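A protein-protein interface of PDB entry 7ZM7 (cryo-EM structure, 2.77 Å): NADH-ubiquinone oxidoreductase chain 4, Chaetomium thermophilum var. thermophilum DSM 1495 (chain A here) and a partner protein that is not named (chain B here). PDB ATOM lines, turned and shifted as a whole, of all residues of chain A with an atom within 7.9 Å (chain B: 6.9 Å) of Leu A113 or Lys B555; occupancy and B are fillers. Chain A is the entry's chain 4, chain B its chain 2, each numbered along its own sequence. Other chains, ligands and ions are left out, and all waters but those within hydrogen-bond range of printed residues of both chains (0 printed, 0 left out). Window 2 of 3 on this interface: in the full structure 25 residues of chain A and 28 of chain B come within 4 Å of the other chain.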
ATOM      1  N   ASN A 110     -21.530  28.846 -39.173  1.00  0.00           N
ATOM      2  CA  ASN A 110     -21.734  28.281 -37.848  1.00  0.00           C
ATOM      3  C   ASN A 110     -22.116  26.805 -37.899  1.00  0.00           C
ATOM      4  O   ASN A 110     -21.522  25.989 -37.189  1.00  0.00           O
ATOM      5  CB  ASN A 110     -22.804  29.068 -37.095  1.00  0.00           C
ATOM      6  CG  ASN A 110     -22.841  28.724 -35.623  1.00  0.00           C
ATOM      7  OD1 ASN A 110     -21.837  28.308 -35.048  1.00  0.00           O
ATOM      8  ND2 ASN A 110     -24.002  28.889 -35.005  1.00  0.00           N
ATOM      9  N   LEU A 111     -23.129  26.463 -38.700  1.00  0.00           N
ATOM     10  CA  LEU A 111     -23.611  25.091 -38.899  1.00  0.00           C
ATOM     11  C   LEU A 111     -23.762  24.319 -37.587  1.00  0.00           C
ATOM     12  O   LEU A 111     -23.705  23.086 -37.575  1.00  0.00           O
ATOM     13  CB  LEU A 111     -22.736  24.296 -39.883  1.00  0.00           C
ATOM     14  CG  LEU A 111     -21.326  23.744 -39.630  1.00  0.00           C
ATOM     15  CD1 LEU A 111     -21.016  22.720 -40.700  1.00  0.00           C
ATOM     16  CD2 LEU A 111     -20.263  24.818 -39.691  1.00  0.00           C
ATOM     17  N   ASP A 112     -23.959  25.021 -36.476  1.00  0.00           N
ATOM     18  CA  ASP A 112     -24.231  24.414 -35.175  1.00  0.00           C
ATOM     19  C   ASP A 112     -25.459  25.130 -34.629  1.00  0.00           C
ATOM     20  O   ASP A 112     -25.347  26.091 -33.866  1.00  0.00           O
ATOM     21  CB  ASP A 112     -23.034  24.533 -34.236  1.00  0.00           C
ATOM     22  N   LEU A 113     -26.596  24.879 -35.149  1.00  0.00           N
ATOM     23  CA  LEU A 113     -27.805  25.682 -34.835  1.00  0.00           C
ATOM     24  C   LEU A 113     -28.335  25.469 -33.422  1.00  0.00           C
ATOM     25  O   LEU A 113     -28.304  24.322 -32.938  1.00  0.00           O
ATOM     26  CB  LEU A 113     -28.891  25.372 -35.870  1.00  0.00           C
ATOM     27  CG  LEU A 113     -28.998  26.354 -37.037  1.00  0.00           C
ATOM     28  CD1 LEU A 113     -27.735  26.347 -37.884  1.00  0.00           C
ATOM     29  CD2 LEU A 113     -30.210  26.032 -37.898  1.00  0.00           C
ATOM     30  N   SER A 114     -28.819  26.419 -32.809  1.00  0.00           N
ATOM     31  CA  SER A 114     -29.430  26.504 -31.497  1.00  0.00           C
ATOM     32  C   SER A 114     -30.703  27.313 -31.642  1.00  0.00           C
ATOM     33  O   SER A 114     -31.248  27.459 -32.737  1.00  0.00           O
ATOM     34  CB  SER A 114     -28.488  27.132 -30.476  1.00  0.00           C
ATOM     35  OG  SER A 114     -29.119  27.331 -29.228  1.00  0.00           O
ATOM     36  N   PHE A 115     -31.196  27.813 -30.518  1.00  0.00           N
ATOM     37  CA  PHE A 115     -32.387  28.647 -30.534  1.00  0.00           C
ATOM     38  C   PHE A 115     -32.025  30.107 -30.771  1.00  0.00           C
ATOM     39  O   PHE A 115     -32.571  30.752 -31.669  1.00  0.00           O
ATOM     40  CB  PHE A 115     -33.147  28.456 -29.228  1.00  0.00           C
ATOM     41  CG  PHE A 115     -33.532  27.035 -28.967  1.00  0.00           C
ATOM     42  CD1 PHE A 115     -32.611  26.128 -28.475  1.00  0.00           C
ATOM     43  CD2 PHE A 115     -34.819  26.596 -29.208  1.00  0.00           C
ATOM     44  CE1 PHE A 115     -32.966  24.820 -28.244  1.00  0.00           C
ATOM     45  CE2 PHE A 115     -35.172  25.286 -28.975  1.00  0.00           C
ATOM     46  CZ  PHE A 115     -34.247  24.401 -28.495  1.00  0.00           C
ATOM     47  N   TYR A 116     -31.073  30.631 -30.010  1.00  0.00           N
ATOM     48  CA  TYR A 116     -30.575  31.991 -30.187  1.00  0.00           C
ATOM     49  C   TYR A 116     -29.082  31.932 -30.483  1.00  0.00           C
ATOM     50  O   TYR A 116     -28.270  31.760 -29.572  1.00  0.00           O
ATOM     51  CB  TYR A 116     -30.864  32.840 -28.955  1.00  0.00           C
ATOM     52  CG  TYR A 116     -32.274  32.680 -28.471  1.00  0.00           C
ATOM     53  CD1 TYR A 116     -33.339  33.195 -29.200  1.00  0.00           C
ATOM     54  CD2 TYR A 116     -32.554  31.995 -27.295  1.00  0.00           C
ATOM     55  CE1 TYR A 116     -34.630  33.034 -28.774  1.00  0.00           C
ATOM     56  CE2 TYR A 116     -33.841  31.828 -26.869  1.00  0.00           C
ATOM     57  CZ  TYR A 116     -34.876  32.350 -27.609  1.00  0.00           C
ATOM     58  OH  TYR A 116     -36.163  32.194 -27.182  1.00  0.00           O
ATOM     59  N   ASP A 117     -28.726  32.088 -31.752  1.00  0.00           N
ATOM     60  CA  ASP A 117     -27.346  32.102 -32.205  1.00  0.00           C
ATOM     61  C   ASP A 117     -26.993  33.456 -32.792  1.00  0.00           C
ATOM     62  O   ASP A 117     -27.739  33.996 -33.608  1.00  0.00           O
ATOM     63  CB  ASP A 117     -27.096  31.031 -33.257  1.00  0.00           C
ATOM     64  CG  ASP A 117     -27.155  29.643 -32.697  1.00  0.00           C
ATOM     65  OD1 ASP A 117     -26.837  29.475 -31.504  1.00  0.00           O
ATOM     66  OD2 ASP A 117     -27.510  28.714 -33.447  1.00  0.00           O
ATOM     67  N   TYR A 119     -25.362  35.699 -35.336  1.00  0.00           N
ATOM     68  CA  TYR A 119     -24.897  35.716 -36.712  1.00  0.00           C
ATOM     69  C   TYR A 119     -24.424  37.121 -37.023  1.00  0.00           C
ATOM     70  O   TYR A 119     -25.219  38.061 -36.991  1.00  0.00           O
ATOM     71  CB  TYR A 119     -26.007  35.312 -37.674  1.00  0.00           C
ATOM     72  CG  TYR A 119     -26.369  33.860 -37.621  1.00  0.00           C
ATOM     73  CD1 TYR A 119     -25.688  32.945 -38.392  1.00  0.00           C
ATOM     74  CD2 TYR A 119     -27.384  33.400 -36.801  1.00  0.00           C
ATOM     75  CE1 TYR A 119     -26.009  31.618 -38.355  1.00  0.00           C
ATOM     76  CE2 TYR A 119     -27.706  32.074 -36.751  1.00  0.00           C
ATOM     77  CZ  TYR A 119     -27.016  31.184 -37.539  1.00  0.00           C
ATOM     78  OH  TYR A 119     -27.305  29.841 -37.524  1.00  0.00           O
ATOM     79  N   THR A 232     -38.298  31.786 -38.703  1.00  0.00           N
ATOM     80  CA  THR A 232     -37.025  32.327 -38.269  1.00  0.00           C
ATOM     81  C   THR A 232     -37.064  33.834 -38.452  1.00  0.00           C
ATOM     82  O   THR A 232     -38.004  34.388 -39.021  1.00  0.00           O
ATOM     83  CB  THR A 232     -35.849  31.660 -39.021  1.00  0.00           C
ATOM     84  OG1 THR A 232     -34.599  32.163 -38.533  1.00  0.00           O
ATOM     85  CG2 THR A 232     -35.931  31.863 -40.511  1.00  0.00           C
ATOM     86  N   PHE B 550     -27.002  33.319 -20.631  1.00  0.00           N
ATOM     87  CA  PHE B 550     -27.955  32.311 -21.172  1.00  0.00           C
ATOM     88  C   PHE B 550     -27.909  32.256 -22.700  1.00  0.00           C
ATOM     89  O   PHE B 550     -28.034  31.156 -23.245  1.00  0.00           O
ATOM     90  CB  PHE B 550     -29.371  32.624 -20.683  1.00  0.00           C
ATOM     91  CG  PHE B 550     -30.472  31.778 -21.270  1.00  0.00           C
ATOM     92  CD1 PHE B 550     -30.709  30.499 -20.799  1.00  0.00           C
ATOM     93  CD2 PHE B 550     -31.277  32.268 -22.285  1.00  0.00           C
ATOM     94  CE1 PHE B 550     -31.721  29.723 -21.340  1.00  0.00           C
ATOM     95  CE2 PHE B 550     -32.287  31.492 -22.825  1.00  0.00           C
ATOM     96  CZ  PHE B 550     -32.508  30.223 -22.349  1.00  0.00           C
ATOM     97  N   PHE B 552     -25.606  32.253 -24.658  1.00  0.00           N
ATOM     98  CA  PHE B 552     -24.477  31.412 -25.117  1.00  0.00           C
ATOM     99  C   PHE B 552     -24.618  29.970 -24.614  1.00  0.00           C
ATOM    100  O   PHE B 552     -23.728  29.168 -24.920  1.00  0.00           O
ATOM    101  CB  PHE B 552     -23.164  32.038 -24.640  1.00  0.00           C
ATOM    102  CG  PHE B 552     -22.987  33.486 -25.011  1.00  0.00           C
ATOM    103  CD1 PHE B 552     -23.087  34.480 -24.054  1.00  0.00           C
ATOM    104  CD2 PHE B 552     -22.726  33.855 -26.319  1.00  0.00           C
ATOM    105  CE1 PHE B 552     -22.925  35.813 -24.398  1.00  0.00           C
ATOM    106  CE2 PHE B 552     -22.567  35.187 -26.663  1.00  0.00           C
ATOM    107  CZ  PHE B 552     -22.667  36.162 -25.702  1.00  0.00           C
ATOM    108  N   MET B 553     -25.678  29.642 -23.869  1.00  0.00           N
ATOM    109  CA  MET B 553     -25.794  28.296 -23.234  1.00  0.00           C
ATOM    110  C   MET B 553     -27.258  27.891 -23.164  1.00  0.00           C
ATOM    111  O   MET B 553     -27.671  27.367 -22.125  1.00  0.00           O
ATOM    112  CB  MET B 553     -25.256  28.319 -21.802  1.00  0.00           C
ATOM    113  CG  MET B 553     -25.628  29.555 -21.034  1.00  0.00           C
ATOM    114  SD  MET B 553     -25.642  29.340 -19.247  1.00  0.00           S
ATOM    115  CE  MET B 553     -27.288  28.671 -19.031  1.00  0.00           C
ATOM    116  N   ASN B 554     -27.984  28.072 -24.255  1.00  0.00           N
ATOM    117  CA  ASN B 554     -29.450  27.836 -24.272  1.00  0.00           C
ATOM    118  C   ASN B 554     -29.882  26.488 -24.869  1.00  0.00           C
ATOM    119  O   ASN B 554     -31.026  26.112 -24.604  1.00  0.00           O
ATOM    120  CB  ASN B 554     -30.168  29.049 -24.882  1.00  0.00           C
ATOM    121  CG  ASN B 554     -29.687  29.421 -26.267  1.00  0.00           C
ATOM    122  OD1 ASN B 554     -30.210  28.932 -27.262  1.00  0.00           O
ATOM    123  ND2 ASN B 554     -28.705  30.302 -26.343  1.00  0.00           N
ATOM    124  N   LYS B 555     -29.023  25.760 -25.579  1.00  0.00           N
ATOM    125  CA  LYS B 555     -29.535  24.538 -26.274  1.00  0.00           C
ATOM    126  C   LYS B 555     -30.065  23.422 -25.357  1.00  0.00           C
ATOM    127  O   LYS B 555     -31.189  23.010 -25.584  1.00  0.00           O
ATOM    128  CB  LYS B 555     -28.585  24.015 -27.352  1.00  0.00           C
ATOM    129  CG  LYS B 555     -29.274  23.257 -28.476  1.00  0.00           C
ATOM    130  CD  LYS B 555     -28.325  22.564 -29.421  1.00  0.00           C
ATOM    131  CE  LYS B 555     -29.058  21.731 -30.448  1.00  0.00           C
ATOM    132  NZ  LYS B 555     -30.148  22.500 -31.092  1.00  0.00           N
ATOM    133  N   GLU B 556     -29.351  23.008 -24.316  1.00  0.00           N
ATOM    134  CA  GLU B 556     -29.811  21.852 -23.497  1.00  0.00           C
ATOM    135  C   GLU B 556     -31.069  22.176 -22.690  1.00  0.00           C
ATOM    136  O   GLU B 556     -31.940  21.306 -22.621  1.00  0.00           O
ATOM    137  CB  GLU B 556     -28.677  21.279 -22.652  1.00  0.00           C
ATOM    138  CG  GLU B 556     -27.702  20.426 -23.441  1.00  0.00           C
ATOM    139  CD  GLU B 556     -26.863  21.177 -24.458  1.00  0.00           C
ATOM    140  OE1 GLU B 556     -25.870  21.809 -24.055  1.00  0.00           O
ATOM    141  OE2 GLU B 556     -27.206  21.132 -25.648  1.00  0.00           O
ATOM    142  N   TRP B 557     -31.150  23.370 -22.110  1.00  0.00           N
ATOM    143  CA  TRP B 557     -32.298  23.789 -21.265  1.00  0.00           C
ATOM    144  C   TRP B 557     -33.577  23.868 -22.107  1.00  0.00           C
ATOM    145  O   TRP B 557     -34.586  23.273 -21.697  1.00  0.00           O
ATOM    146  CB  TRP B 557     -31.940  25.092 -20.534  1.00  0.00           C
ATOM    147  CG  TRP B 557     -32.840  25.585 -19.444  1.00  0.00           C
ATOM    148  CD1 TRP B 557     -34.050  25.094 -19.058  1.00  0.00           C
ATOM    149  CD2 TRP B 557     -32.576  26.710 -18.589  1.00  0.00           C
ATOM    150  NE1 TRP B 557     -34.557  25.835 -18.025  1.00  0.00           N
ATOM    151  CE2 TRP B 557     -33.672  26.830 -17.713  1.00  0.00           C
ATOM    152  CE3 TRP B 557     -31.519  27.619 -18.475  1.00  0.00           C
ATOM    153  CZ2 TRP B 557     -33.739  27.828 -16.743  1.00  0.00           C
ATOM    154  CZ3 TRP B 557     -31.585  28.602 -17.516  1.00  0.00           C
ATOM    155  CH2 TRP B 557     -32.681  28.703 -16.661  1.00  0.00           C
ATOM    156  N   LEU B 558     -33.537  24.566 -23.241  1.00  0.00           N
ATOM    157  CA  LEU B 558     -34.753  24.726 -24.077  1.00  0.00           C
ATOM    158  C   LEU B 558     -35.118  23.414 -24.777  1.00  0.00           C
ATOM    159  O   LEU B 558     -36.319  23.150 -24.913  1.00  0.00           O
ATOM    160  CB  LEU B 558     -34.571  25.909 -25.030  1.00  0.00           C
ATOM    161  CG  LEU B 558     -34.458  27.272 -24.350  1.00  0.00           C
ATOM    162  CD1 LEU B 558     -34.023  28.342 -25.337  1.00  0.00           C
ATOM    163  CD2 LEU B 558     -35.774  27.653 -23.690  1.00  0.00           C
ATOM    164  N   SER B 559     -34.124  22.640 -25.213  1.00  0.00           N
ATOM    165  CA  SER B 559     -34.356  21.330 -25.887  1.00  0.00           C
ATOM    166  C   SER B 559     -35.038  20.341 -24.941  1.00  0.00           C
ATOM    167  O   SER B 559     -35.855  19.561 -25.415  1.00  0.00           O
ATOM    168  CB  SER B 559     -33.089  20.765 -26.457  1.00  0.00           C
ATOM    169  OG  SER B 559     -32.714  21.451 -27.639  1.00  0.00           O
ATOM    170  N   MET B 560     -34.702  20.375 -23.654  1.00  0.00           N
ATOM    171  CA  MET B 560     -35.340  19.490 -22.654  1.00  0.00           C
ATOM    172  C   MET B 560     -36.829  19.791 -22.647  1.00  0.00           C
ATOM    173  O   MET B 560     -37.612  18.845 -22.647  1.00  0.00           O
ATOM    174  CB  MET B 560     -34.781  19.849 -21.275  1.00  0.00           C
ATOM    175  CG  MET B 560     -35.429  19.123 -20.123  1.00  0.00           C
ATOM    176  SD  MET B 560     -35.003  19.937 -18.570  1.00  0.00           S
ATOM    177  CE  MET B 560     -36.337  21.124 -18.451  1.00  0.00           C
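The side-chain amino group (NZ) of Lys B555 sits at hydrogen-bond distance from the backbone carbonyl oxygen (O) of Leu A113 (3.2 Å). The side-chain amide oxygen of Asn B554 is in hydrogen-bond range of the backbone NH of Tyr A116. OD1 of Asn B554 lies within hydrogen-bond range of OG of Ser A114 (2.8 Å).
The backbone carbonyl oxygen (O) of Lys B555 lies within hydrogen-bond range of the side-chain hydroxyl (OG) of Ser B559. The backbone carbonyl oxygen (O) of Phe B550 sits at hydrogen-bond distance from the side-chain amide nitrogen (ND2) of Asn B554 (3.3 Å). N of Ser A114 is in hydrogen-bond range of OD2 of Asp A117 (2.7 Å).
Lys B555 touches Ser A114. Asn B554 touches Phe A115 (OD1 to CB, 3.6 Å). Lys B555 touches Phe A115 (O to CE1, 3.7 Å). CE1 of Phe A115 touches CB of Leu B558, at 3.8 Å. Ser B559 touches Phe A115 (OG to CE1, 3.4 Å). Tyr A116 touches Leu B558 (CE2 to CD1, 3.8 Å).
Of the printed residues of chain B, Ser A114 touches Asn B554 and Lys B555. Of the printed residues of chain B, Phe A115 touches Asn B554, Lys B555, Leu B558 and Ser B559. Printed residues of chain B within 4 Å of Tyr A116: Asn B554 and Leu B558. Printed residues of chain A within 4 Å of Asn B554: Ser A114, Phe A115 and Tyr A116. Of chain A, only Leu A113, Ser A114 and Phe A115 come within 4 Å of Lys B555. Of the printed residues of chain A, Ser B559 touches Phe A115. The nearest residue of chain A that does not touch Lys B555 is Asp A112 (6.4 Å). The nearest printed residue of chain B that does not touch Ser A114 is Leu B558 (6.3 Å).
Of the 10 printed residues of chain A, 4 touch a printed residue of chain B. Of the 10 printed residues of chain B, 4 touch a printed residue of chain A. Among the printed residues, 9 pairs touch across the chains. Among the printed residues, no Asp or Glu carboxylate lies within 4 Å of a Lys or Arg side-chain nitrogen of the other chain.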
